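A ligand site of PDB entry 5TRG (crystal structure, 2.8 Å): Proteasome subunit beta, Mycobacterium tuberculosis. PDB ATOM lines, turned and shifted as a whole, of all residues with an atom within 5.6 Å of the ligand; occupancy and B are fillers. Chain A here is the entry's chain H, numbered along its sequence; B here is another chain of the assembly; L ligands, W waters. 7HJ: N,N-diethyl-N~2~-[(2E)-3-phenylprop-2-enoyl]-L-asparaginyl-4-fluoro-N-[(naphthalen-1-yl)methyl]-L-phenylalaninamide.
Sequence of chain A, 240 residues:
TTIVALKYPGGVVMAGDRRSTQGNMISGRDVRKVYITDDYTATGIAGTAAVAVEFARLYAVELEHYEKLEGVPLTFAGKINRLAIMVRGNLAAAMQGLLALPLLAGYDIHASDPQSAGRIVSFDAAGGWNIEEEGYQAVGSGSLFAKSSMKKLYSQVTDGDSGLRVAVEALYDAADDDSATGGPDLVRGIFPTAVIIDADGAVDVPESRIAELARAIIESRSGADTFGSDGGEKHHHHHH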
ATOM      1  N   THR A   1      -7.165  18.112  -0.383  1.00  0.00           N
ATOM      2  CA  THR A   1      -6.440  19.239   0.208  1.00  0.00           C
ATOM      3  C   THR A   1      -5.645  19.987  -0.841  1.00  0.00           C
ATOM      4  O   THR A   1      -5.066  19.406  -1.737  1.00  0.00           O
ATOM      5  CB  THR A   1      -5.480  18.767   1.321  1.00  0.00           C
ATOM      6  OG1 THR A   1      -6.236  18.281   2.411  1.00  0.00           O
ATOM      7  CG2 THR A   1      -4.602  19.875   1.840  1.00  0.00           C
ATOM      8  N   ARG A  19     -11.706  21.530   3.471  1.00  0.00           N
ATOM      9  CA  ARG A  19     -12.357  20.239   3.295  1.00  0.00           C
ATOM     10  C   ARG A  19     -11.618  19.105   3.945  1.00  0.00           C
ATOM     11  O   ARG A  19     -10.393  19.028   3.897  1.00  0.00           O
ATOM     12  CB  ARG A  19     -12.525  19.920   1.810  1.00  0.00           C
ATOM     13  CG  ARG A  19     -13.005  18.490   1.552  1.00  0.00           C
ATOM     14  CD  ARG A  19     -13.605  18.322   0.208  1.00  0.00           C
ATOM     15  NE  ARG A  19     -14.826  19.080   0.089  1.00  0.00           N
ATOM     16  CZ  ARG A  19     -15.513  19.167  -1.036  1.00  0.00           C
ATOM     17  NH1 ARG A  19     -15.080  18.548  -2.112  1.00  0.00           N
ATOM     18  NH2 ARG A  19     -16.619  19.890  -1.082  1.00  0.00           N
ATOM     19  N   SER A  20     -12.373  18.166   4.506  1.00  0.00           N
ATOM     20  CA  SER A  20     -11.848  16.921   5.034  1.00  0.00           C
ATOM     21  C   SER A  20     -12.650  15.761   4.480  1.00  0.00           C
ATOM     22  O   SER A  20     -13.874  15.767   4.558  1.00  0.00           O
ATOM     23  CB  SER A  20     -11.923  16.922   6.551  1.00  0.00           C
ATOM     24  OG  SER A  20     -11.651  15.644   7.047  1.00  0.00           O
ATOM     25  N   THR A  21     -11.967  14.725   3.986  1.00  0.00           N
ATOM     26  CA  THR A  21     -12.623  13.577   3.392  1.00  0.00           C
ATOM     27  C   THR A  21     -12.254  12.272   4.103  1.00  0.00           C
ATOM     28  O   THR A  21     -11.214  12.156   4.745  1.00  0.00           O
ATOM     29  CB  THR A  21     -12.270  13.430   1.908  1.00  0.00           C
ATOM     30  OG1 THR A  21     -10.849  13.449   1.768  1.00  0.00           O
ATOM     31  CG2 THR A  21     -12.893  14.486   1.063  1.00  0.00           C
ATOM     32  N   GLN A  22     -13.138  11.291   3.943  1.00  0.00           N
ATOM     33  CA  GLN A  22     -12.906   9.894   4.310  1.00  0.00           C
ATOM     34  C   GLN A  22     -13.345   9.099   3.105  1.00  0.00           C
ATOM     35  O   GLN A  22     -14.521   8.743   2.996  1.00  0.00           O
ATOM     36  CB  GLN A  22     -13.651   9.474   5.526  1.00  0.00           C
ATOM     37  CG  GLN A  22     -12.875   9.739   6.749  1.00  0.00           C
ATOM     38  CD  GLN A  22     -13.641   9.359   7.958  1.00  0.00           C
ATOM     39  OE1 GLN A  22     -14.355   8.350   7.965  1.00  0.00           O
ATOM     40  NE2 GLN A  22     -13.499  10.160   9.022  1.00  0.00           N
ATOM     41  N   GLY A  23     -12.406   8.799   2.227  1.00  0.00           N
ATOM     42  CA  GLY A  23     -12.724   8.239   0.931  1.00  0.00           C
ATOM     43  C   GLY A  23     -13.388   9.306   0.093  1.00  0.00           C
ATOM     44  O   GLY A  23     -12.832  10.391  -0.128  1.00  0.00           O
ATOM     45  N   SER A  27     -16.185  14.494   5.346  1.00  0.00           N
ATOM     46  CA  SER A  27     -16.232  14.388   6.805  1.00  0.00           C
ATOM     47  C   SER A  27     -15.938  15.688   7.512  1.00  0.00           C
ATOM     48  O   SER A  27     -16.009  15.730   8.736  1.00  0.00           O
ATOM     49  CB  SER A  27     -15.253  13.323   7.278  1.00  0.00           C
ATOM     50  OG  SER A  27     -13.931  13.650   6.910  1.00  0.00           O
ATOM     51  N   VAL A  31     -12.280  22.587   8.357  1.00  0.00           N
ATOM     52  CA  VAL A  31     -11.027  22.305   8.989  1.00  0.00           C
ATOM     53  C   VAL A  31     -10.013  23.364   8.624  1.00  0.00           C
ATOM     54  O   VAL A  31     -10.146  24.075   7.633  1.00  0.00           O
ATOM     55  CB  VAL A  31     -10.526  20.909   8.603  1.00  0.00           C
ATOM     56  CG1 VAL A  31     -11.657  19.916   8.746  1.00  0.00           C
ATOM     57  CG2 VAL A  31     -10.075  20.947   7.224  1.00  0.00           C
ATOM     58  N   ARG A  32      -9.016  23.527   9.488  1.00  0.00           N
ATOM     59  CA  ARG A  32      -7.953  24.502   9.324  1.00  0.00           C
ATOM     60  C   ARG A  32      -6.660  23.762   9.020  1.00  0.00           C
ATOM     61  O   ARG A  32      -6.285  22.850   9.755  1.00  0.00           O
ATOM     62  CB  ARG A  32      -7.789  25.384  10.560  1.00  0.00           C
ATOM     63  CG  ARG A  32      -8.722  26.604  10.577  1.00  0.00           C
ATOM     64  CD  ARG A  32      -9.430  26.841  11.932  1.00  0.00           C
ATOM     65  NE  ARG A  32     -10.338  25.750  12.319  1.00  0.00           N
ATOM     66  CZ  ARG A  32     -11.236  25.828  13.300  1.00  0.00           C
ATOM     67  NH1 ARG A  32     -11.998  24.777  13.602  1.00  0.00           N
ATOM     68  NH2 ARG A  32     -11.363  26.965  13.969  1.00  0.00           N
ATOM     69  N   LYS A  33      -6.015  24.136   7.935  1.00  0.00           N
ATOM     70  CA  LYS A  33      -4.816  23.467   7.494  1.00  0.00           C
ATOM     71  C   LYS A  33      -3.595  24.358   7.468  1.00  0.00           C
ATOM     72  O   LYS A  33      -2.510  23.887   7.134  1.00  0.00           O
ATOM     73  CB  LYS A  33      -5.044  22.859   6.111  1.00  0.00           C
ATOM     74  CG  LYS A  33      -6.278  22.007   6.045  1.00  0.00           C
ATOM     75  CD  LYS A  33      -6.509  21.487   4.680  1.00  0.00           C
ATOM     76  CE  LYS A  33      -7.824  20.793   4.589  1.00  0.00           C
ATOM     77  NZ  LYS A  33      -7.903  20.059   3.309  1.00  0.00           N
ATOM     78  N   TYR A  35      -1.343  27.031   9.795  1.00  0.00           N
ATOM     79  CA  TYR A  35      -1.128  27.429  11.174  1.00  0.00           C
ATOM     80  C   TYR A  35      -0.022  28.455  11.256  1.00  0.00           C
ATOM     81  O   TYR A  35       1.009  28.331  10.596  1.00  0.00           O
ATOM     82  CB  TYR A  35      -0.744  26.243  12.040  1.00  0.00           C
ATOM     83  CG  TYR A  35      -1.816  25.202  12.046  1.00  0.00           C
ATOM     84  CD1 TYR A  35      -1.822  24.211  11.109  1.00  0.00           C
ATOM     85  CD2 TYR A  35      -2.836  25.219  12.975  1.00  0.00           C
ATOM     86  CE1 TYR A  35      -2.813  23.235  11.097  1.00  0.00           C
ATOM     87  CE2 TYR A  35      -3.831  24.251  12.967  1.00  0.00           C
ATOM     88  CZ  TYR A  35      -3.803  23.261  12.016  1.00  0.00           C
ATOM     89  OH  TYR A  35      -4.766  22.281  11.959  1.00  0.00           O
ATOM     90  N   ILE A  45      -0.300  21.998   6.025  1.00  0.00           N
ATOM     91  CA  ILE A  45       0.008  20.579   5.923  1.00  0.00           C
ATOM     92  C   ILE A  45      -1.103  19.816   5.199  1.00  0.00           C
ATOM     93  O   ILE A  45      -2.292  20.049   5.433  1.00  0.00           O
ATOM     94  CB  ILE A  45       0.257  19.989   7.312  1.00  0.00           C
ATOM     95  CG1 ILE A  45       1.099  20.968   8.120  1.00  0.00           C
ATOM     96  CG2 ILE A  45       0.981  18.665   7.195  1.00  0.00           C
ATOM     97  CD1 ILE A  45       1.510  20.468   9.451  1.00  0.00           C
ATOM     98  N   ALA A  46      -0.712  18.850   4.373  1.00  0.00           N
ATOM     99  CA  ALA A  46      -1.653  18.002   3.649  1.00  0.00           C
ATOM    100  C   ALA A  46      -1.442  16.554   4.053  1.00  0.00           C
ATOM    101  O   ALA A  46      -0.339  16.131   4.388  1.00  0.00           O
ATOM    102  CB  ALA A  46      -1.461  18.138   2.166  1.00  0.00           C
ATOM    103  N   GLY A  47      -2.501  15.789   4.053  1.00  0.00           N
ATOM    104  CA  GLY A  47      -2.296  14.402   4.415  1.00  0.00           C
ATOM    105  C   GLY A  47      -3.289  13.990   5.433  1.00  0.00           C
ATOM    106  O   GLY A  47      -4.381  14.554   5.545  1.00  0.00           O
ATOM    107  N   THR A  48      -2.956  12.960   6.196  1.00  0.00           N
ATOM    108  CA  THR A  48      -3.880  12.502   7.214  1.00  0.00           C
ATOM    109  C   THR A  48      -3.937  13.517   8.345  1.00  0.00           C
ATOM    110  O   THR A  48      -2.911  14.037   8.784  1.00  0.00           O
ATOM    111  CB  THR A  48      -3.486  11.141   7.726  1.00  0.00           C
ATOM    112  OG1 THR A  48      -2.588  11.331   8.787  1.00  0.00           O
ATOM    113  CG2 THR A  48      -2.794  10.374   6.664  1.00  0.00           C
ATOM    114  N   ALA A  49      -5.145  13.819   8.782  1.00  0.00           N
ATOM    115  CA  ALA A  49      -5.378  14.919   9.713  1.00  0.00           C
ATOM    116  C   ALA A  49      -4.547  14.752  10.979  1.00  0.00           C
ATOM    117  O   ALA A  49      -3.892  15.692  11.420  1.00  0.00           O
ATOM    118  CB  ALA A  49      -6.857  14.999  10.048  1.00  0.00           C
ATOM    119  N   ALA A  50      -4.561  13.551  11.547  1.00  0.00           N
ATOM    120  CA  ALA A  50      -3.862  13.293  12.795  1.00  0.00           C
ATOM    121  C   ALA A  50      -2.391  13.660  12.702  1.00  0.00           C
ATOM    122  O   ALA A  50      -1.848  14.381  13.556  1.00  0.00           O
ATOM    123  CB  ALA A  50      -4.024  11.826  13.173  1.00  0.00           C
ATOM    124  N   ALA A  52      -0.962  15.581  10.387  1.00  0.00           N
ATOM    125  CA  ALA A  52      -0.799  16.980  10.029  1.00  0.00           C
ATOM    126  C   ALA A  52      -0.857  17.873  11.257  1.00  0.00           C
ATOM    127  O   ALA A  52       0.002  18.723  11.471  1.00  0.00           O
ATOM    128  CB  ALA A  52      -1.886  17.391   9.045  1.00  0.00           C
ATOM    129  N   VAL A  53      -1.873  17.663  12.090  1.00  0.00           N
ATOM    130  CA  VAL A  53      -2.045  18.477  13.292  1.00  0.00           C
ATOM    131  C   VAL A  53      -0.921  18.250  14.291  1.00  0.00           C
ATOM    132  O   VAL A  53      -0.376  19.210  14.832  1.00  0.00           O
ATOM    133  CB  VAL A  53      -3.439  18.184  13.877  1.00  0.00           C
ATOM    134  CG1 VAL A  53      -3.586  18.769  15.276  1.00  0.00           C
ATOM    135  CG2 VAL A  53      -4.482  18.781  12.950  1.00  0.00           C
ATOM    136  N   GLY A  97       0.755   4.482   5.834  1.00  0.00           N
ATOM    137  CA  GLY A  97      -0.445   5.215   5.493  1.00  0.00           C
ATOM    138  C   GLY A  97      -0.673   6.479   6.287  1.00  0.00           C
ATOM    139  O   GLY A  97      -1.616   7.216   5.968  1.00  0.00           O
ATOM    140  N   LEU A  98       0.127   6.774   7.307  1.00  0.00           N
ATOM    141  CA  LEU A  98      -0.038   8.009   8.075  1.00  0.00           C
ATOM    142  C   LEU A  98       0.860   9.106   7.501  1.00  0.00           C
ATOM    143  O   LEU A  98       1.698   9.685   8.177  1.00  0.00           O
ATOM    144  CB  LEU A  98       0.281   7.768   9.542  1.00  0.00           C
ATOM    145  CG  LEU A  98      -0.520   6.734  10.318  1.00  0.00           C
ATOM    146  CD1 LEU A  98      -0.118   6.788  11.768  1.00  0.00           C
ATOM    147  CD2 LEU A  98      -1.994   7.008  10.178  1.00  0.00           C
ATOM    148  N   LEU A  99       0.637   9.432   6.244  1.00  0.00           N
ATOM    149  CA  LEU A  99       1.530  10.343   5.545  1.00  0.00           C
ATOM    150  C   LEU A  99       1.011  11.758   5.633  1.00  0.00           C
ATOM    151  O   LEU A  99      -0.200  11.978   5.547  1.00  0.00           O
ATOM    152  CB  LEU A  99       1.682   9.932   4.077  1.00  0.00           C
ATOM    153  CG  LEU A  99       2.289  11.028   3.201  1.00  0.00           C
ATOM    154  CD1 LEU A  99       3.771  11.202   3.508  1.00  0.00           C
ATOM    155  CD2 LEU A  99       2.054  10.680   1.755  1.00  0.00           C
ATOM    156  N   LEU B  91      -3.866   2.462  17.986  1.00  0.00           N
ATOM    157  CA  LEU B  91      -3.873   2.282  16.534  1.00  0.00           C
ATOM    158  C   LEU B  91      -3.322   0.930  16.105  1.00  0.00           C
ATOM    159  O   LEU B  91      -3.876   0.279  15.211  1.00  0.00           O
ATOM    160  CB  LEU B  91      -3.099   3.395  15.859  1.00  0.00           C
ATOM    161  CG  LEU B  91      -3.115   3.224  14.337  1.00  0.00           C
ATOM    162  CD1 LEU B  91      -4.507   2.925  13.758  1.00  0.00           C
ATOM    163  CD2 LEU B  91      -2.580   4.462  13.682  1.00  0.00           C
ATOM    164  N   MET B  95      -5.612  -1.773  13.866  1.00  0.00           N
ATOM    165  CA  MET B  95      -5.349  -2.379  12.567  1.00  0.00           C
ATOM    166  C   MET B  95      -5.463  -3.900  12.585  1.00  0.00           C
ATOM    167  O   MET B  95      -5.632  -4.501  11.526  1.00  0.00           O
ATOM    168  CB  MET B  95      -3.965  -1.951  12.058  1.00  0.00           C
ATOM    169  CG  MET B  95      -3.808  -0.470  11.791  1.00  0.00           C
ATOM    170  SD  MET B  95      -4.785   0.082  10.378  1.00  0.00           S
ATOM    171  CE  MET B  95      -6.421   0.487  11.056  1.00  0.00           C
ATOM    172  N   SER B 122     -15.551  14.677  17.264  1.00  0.00           N
ATOM    173  CA  SER B 122     -15.396  13.375  16.622  1.00  0.00           C
ATOM    174  C   SER B 122     -13.922  13.021  16.461  1.00  0.00           C
ATOM    175  O   SER B 122     -13.029  13.881  16.475  1.00  0.00           O
ATOM    176  CB  SER B 122     -16.093  13.348  15.270  1.00  0.00           C
ATOM    177  OG  SER B 122     -15.722  14.466  14.495  1.00  0.00           O
ATOM    178  N   PHE B 123     -13.675  11.717  16.350  1.00  0.00           N
ATOM    179  CA  PHE B 123     -12.331  11.166  16.262  1.00  0.00           C
ATOM    180  C   PHE B 123     -12.239  10.126  15.152  1.00  0.00           C
ATOM    181  O   PHE B 123     -13.226   9.494  14.810  1.00  0.00           O
ATOM    182  CB  PHE B 123     -11.917  10.541  17.542  1.00  0.00           C
ATOM    183  CG  PHE B 123     -11.809  11.482  18.665  1.00  0.00           C
ATOM    184  CD1 PHE B 123     -12.928  11.894  19.363  1.00  0.00           C
ATOM    185  CD2 PHE B 123     -10.574  11.959  19.051  1.00  0.00           C
ATOM    186  CE1 PHE B 123     -12.803  12.769  20.431  1.00  0.00           C
ATOM    187  CE2 PHE B 123     -10.446  12.829  20.107  1.00  0.00           C
ATOM    188  CZ  PHE B 123     -11.556  13.249  20.796  1.00  0.00           C
ATOM    189  N   ASP B 124     -11.045   9.955  14.601  1.00  0.00           N
ATOM    190  CA  ASP B 124     -10.758   8.856  13.687  1.00  0.00           C
ATOM    191  C   ASP B 124      -9.801   7.883  14.361  1.00  0.00           C
ATOM    192  O   ASP B 124      -9.298   8.125  15.463  1.00  0.00           O
ATOM    193  CB  ASP B 124     -10.205   9.359  12.346  1.00  0.00           C
ATOM    194  CG  ASP B 124      -8.790   9.949  12.447  1.00  0.00           C
ATOM    195  OD1 ASP B 124      -8.003   9.603  13.352  1.00  0.00           O
ATOM    196  OD2 ASP B 124      -8.470  10.792  11.587  1.00  0.00           O
ATOM    197  N   ALA B 125      -9.544   6.761  13.685  1.00  0.00           N
ATOM    198  CA  ALA B 125      -8.763   5.713  14.360  1.00  0.00           C
ATOM    199  C   ALA B 125      -7.317   6.091  14.621  1.00  0.00           C
ATOM    200  O   ALA B 125      -6.658   5.387  15.389  1.00  0.00           O
ATOM    201  CB  ALA B 125      -8.839   4.396  13.607  1.00  0.00           C
ATOM    202  N   ALA B 126      -6.797   7.137  14.001  1.00  0.00           N
ATOM    203  CA  ALA B 126      -5.414   7.556  14.217  1.00  0.00           C
ATOM    204  C   ALA B 126      -5.312   8.698  15.217  1.00  0.00           C
ATOM    205  O   ALA B 126      -4.235   9.252  15.388  1.00  0.00           O
ATOM    206  CB  ALA B 126      -4.761   7.970  12.912  1.00  0.00           C
ATOM    207  N   GLY B 128      -7.047  11.636  15.024  1.00  0.00           N
ATOM    208  CA  GLY B 128      -7.531  12.910  14.512  1.00  0.00           C
ATOM    209  C   GLY B 128      -8.922  13.223  15.033  1.00  0.00           C
ATOM    210  O   GLY B 128      -9.784  12.348  15.138  1.00  0.00           O
ATOM    211  N   TRP B 129      -9.138  14.495  15.374  1.00  0.00           N
ATOM    212  CA  TRP B 129     -10.375  14.954  15.961  1.00  0.00           C
ATOM    213  C   TRP B 129     -10.841  16.208  15.241  1.00  0.00           C
ATOM    214  O   TRP B 129     -10.056  16.959  14.679  1.00  0.00           O
ATOM    215  CB  TRP B 129     -10.226  15.224  17.451  1.00  0.00           C
ATOM    216  CG  TRP B 129      -9.038  16.052  17.798  1.00  0.00           C
ATOM    217  CD1 TRP B 129      -7.793  15.607  18.082  1.00  0.00           C
ATOM    218  CD2 TRP B 129      -8.992  17.469  17.890  1.00  0.00           C
ATOM    219  NE1 TRP B 129      -6.958  16.663  18.355  1.00  0.00           N
ATOM    220  CE2 TRP B 129      -7.665  17.823  18.227  1.00  0.00           C
ATOM    221  CE3 TRP B 129      -9.933  18.480  17.713  1.00  0.00           C
ATOM    222  CZ2 TRP B 129      -7.244  19.142  18.402  1.00  0.00           C
ATOM    223  CZ3 TRP B 129      -9.526  19.802  17.889  1.00  0.00           C
ATOM    224  CH2 TRP B 129      -8.193  20.124  18.226  1.00  0.00           C
ATOM    225  N   ASN B 130     -12.156  16.413  15.265  1.00  0.00           N
ATOM    226  CA  ASN B 130     -12.745  17.649  14.761  1.00  0.00           C
ATOM    227  C   ASN B 130     -13.819  18.102  15.733  1.00  0.00           C
ATOM    228  O   ASN B 130     -14.682  17.313  16.120  1.00  0.00           O
ATOM    229  CB  ASN B 130     -13.343  17.463  13.369  1.00  0.00           C
ATOM    230  CG  ASN B 130     -13.662  18.791  12.703  1.00  0.00           C
ATOM    231  OD1 ASN B 130     -12.872  19.733  12.763  1.00  0.00           O
ATOM    232  ND2 ASN B 130     -14.819  18.870  12.081  1.00  0.00           N
HETATM  233  C37 7HJ L   1      -9.410   9.197   8.073  1.00  0.00           C
HETATM  234  O46 7HJ L   1      -9.843   9.042   6.940  1.00  0.00           O
HETATM  235  C38 7HJ L   1      -8.913   8.021   8.889  1.00  0.00           C
HETATM  236  C39 7HJ L   1      -7.601   7.416   8.449  1.00  0.00           C
HETATM  237  C40 7HJ L   1      -7.185   6.193   9.173  1.00  0.00           C
HETATM  238  C41 7HJ L   1      -6.485   6.307  10.363  1.00  0.00           C
HETATM  239  C42 7HJ L   1      -6.111   5.186  11.072  1.00  0.00           C
HETATM  240  C43 7HJ L   1      -6.435   3.900  10.636  1.00  0.00           C
HETATM  241  C44 7HJ L   1      -7.160   3.766   9.462  1.00  0.00           C
HETATM  242  C45 7HJ L   1      -7.530   4.899   8.757  1.00  0.00           C
HETATM  243  O01 7HJ L   1      -7.526  12.360   7.720  1.00  0.00           O
HETATM  244  C02 7HJ L   1      -8.598  12.331   7.160  1.00  0.00           C
HETATM  245  C27 7HJ L   1      -9.805  11.736   7.958  1.00  0.00           C
HETATM  246  C28 7HJ L   1     -10.140  12.865   8.981  1.00  0.00           C
HETATM  247  C29 7HJ L   1     -11.514  12.911   9.624  1.00  0.00           C
HETATM  248  N30 7HJ L   1     -11.608  13.378  11.000  1.00  0.00           N
HETATM  249  C31 7HJ L   1     -12.897  13.434  11.649  1.00  0.00           C
HETATM  250  C32 7HJ L   1     -13.564  12.094  11.965  1.00  0.00           C
HETATM  251  C33 7HJ L   1     -10.446  13.772  11.819  1.00  0.00           C
HETATM  252  C34 7HJ L   1     -10.123  15.242  11.671  1.00  0.00           C
HETATM  253  O35 7HJ L   1     -12.503  12.586   9.012  1.00  0.00           O
HETATM  254  N36 7HJ L   1      -9.387  10.496   8.634  1.00  0.00           N
HETATM  255  N03 7HJ L   1      -8.704  12.803   5.878  1.00  0.00           N
HETATM  256  C04 7HJ L   1      -7.629  13.356   5.152  1.00  0.00           C
HETATM  257  C05 7HJ L   1      -7.853  14.790   4.987  1.00  0.00           C
HETATM  258  O18 7HJ L   1      -8.984  15.175   4.811  1.00  0.00           O
HETATM  259  C19 7HJ L   1      -7.537  12.656   3.784  1.00  0.00           C
HETATM  260  C20 7HJ L   1      -7.014  11.259   3.945  1.00  0.00           C
HETATM  261  C21 7HJ L   1      -7.870  10.162   4.167  1.00  0.00           C
HETATM  262  C26 7HJ L   1      -5.648  11.010   3.986  1.00  0.00           C
HETATM  263  C22 7HJ L   1      -7.373   8.894   4.362  1.00  0.00           C
HETATM  264  C25 7HJ L   1      -5.112   9.756   4.172  1.00  0.00           C
HETATM  265  C23 7HJ L   1      -5.991   8.707   4.359  1.00  0.00           C
HETATM  266  F24 7HJ L   1      -5.462   7.488   4.536  1.00  0.00           F
HETATM  267  C11 7HJ L   1      -5.440  19.267   8.568  1.00  0.00           C
HETATM  268  C10 7HJ L   1      -4.686  19.270   7.447  1.00  0.00           C
HETATM  269  C12 7HJ L   1      -6.671  18.586   8.601  1.00  0.00           C
HETATM  270  C14 7HJ L   1      -8.370  17.270   7.568  1.00  0.00           C
HETATM  271  C13 7HJ L   1      -7.106  17.919   7.480  1.00  0.00           C
HETATM  272  C15 7HJ L   1      -9.142  17.280   8.695  1.00  0.00           C
HETATM  273  N06 7HJ L   1      -6.785  15.665   5.128  1.00  0.00           N
HETATM  274  C07 7HJ L   1      -6.826  17.146   5.047  1.00  0.00           C
HETATM  275  C08 7HJ L   1      -6.346  17.899   6.298  1.00  0.00           C
HETATM  276  C09 7HJ L   1      -5.138  18.572   6.317  1.00  0.00           C
HETATM  277  C16 7HJ L   1      -8.686  17.970   9.821  1.00  0.00           C
HETATM  278  C17 7HJ L   1      -7.463  18.607   9.765  1.00  0.00           C
HETATM  279  O   HOH W   1     -10.891   6.109  10.938  1.00  0.00           O
HETATM  280  O   HOH W   2      -6.085  11.383  10.568  1.00  0.00           O
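The backbone carbonyl oxygen (O) of Arg 32 lies within hydrogen-bond range of the side-chain hydroxyl (OH) of Tyr 35 (2.7 Å).
The backbone NH of Gly 128 of chain B sits at hydrogen-bond distance from the side-chain carboxylate of Asp 124 of chain B, 2.8 Å away.
The side-chain hydroxyl of Thr 1 sits at hydrogen-bond distance from the side-chain amino group of Lys 33, 2.6 Å away.
N of Ser 27 sits at hydrogen-bond distance from O of Ser 20, 2.8 Å away.
The backbone NH (N) of Thr 48 lies within hydrogen-bond range of the backbone carbonyl oxygen (O) of Leu 99.
O of Lys 33 is in hydrogen-bond range of N of Ile 45 (3.1 Å).
N of Ala 126 of chain B is in hydrogen-bond range of OD1 of Asp 124 of chain B.
The backbone carbonyl oxygen (O) of Arg 19 sits at hydrogen-bond distance from the side-chain amino group (NZ) of Lys 33, at 2.8 Å.
Water W2 lies within hydrogen-bond range of OD2 of Asp 124 of chain B (2.7 Å), N of Ala 50 (2.8 Å), N of Ala 49 (3.2 Å) and O01 of the ligand (3.3 Å).
A nitrogen (N03) of the ligand is in hydrogen-bond range of the backbone carbonyl oxygen (O) of Thr 21, at 2.8 Å.
The backbone carbonyl oxygen (O) of Gly 47 sits at hydrogen-bond distance from a nitrogen (N06) of the ligand (2.7 Å).
The side-chain amide nitrogen (NE2) of Gln 22 sits at hydrogen-bond distance from an oxygen (O35) of the ligand, at 2.6 Å.
An oxygen (O01) of the ligand lies within hydrogen-bond range of the backbone NH (N) of Ala 49 (3.0 Å).
O35 of the ligand is in hydrogen-bond range of OG of Ser 27, 2.8 Å away.
An oxygen (O18) of the ligand lies within hydrogen-bond range of the backbone NH (N) of Thr 21 (3.1 Å).
OD2 of Asp 124 of chain B is in hydrogen-bond range of N36 of the ligand, 3.1 Å away.
Merely in contact with the ligand: Thr 1 (2.9 Å), Ser 20 (3.4 Å), Val 31 (3.6 Å), Arg 32 (3.9 Å), Lys 33 (3.5 Å), Ile 45 (3.2 Å), Thr 48 (3.5 Å), Ala 52 (3.7 Å), Leu 91 of chain B (3.8 Å), Met 95 of chain B (3.4 Å), Phe 123 of chain B (3.9 Å), Ala 125 of chain B (3.8 Å), Ala 126 of chain B (3.5 Å), Gly 128 of chain B (3.6 Å) and Trp 129 of chain B (3.5 Å).
Hydrophobic or aromatic side chains within 4 Å of the ligand: Val 31, Ala 49, Ala 52, Leu 91 of chain B, Met 95 of chain B, Ala 125 of chain B and Ala 126 of chain B.
Within 4 Å of the ligand: Thr 1, Ser 20, Thr 21, Gln 22, Ser 27, Val 31, Arg 32, Lys 33, Ile 45, Gly 47, Thr 48, Ala 49, Ala 52, Leu 91 of chain B, Met 95 of chain B, Phe 123 of chain B, Asp 124 of chain B, Ala 125 of chain B, Ala 126 of chain B, Gly 128 of chain B and Trp 129 of chain B.
The nearest printed residue that does not touch the ligand is Ser 122 of chain B (4.1 Å).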
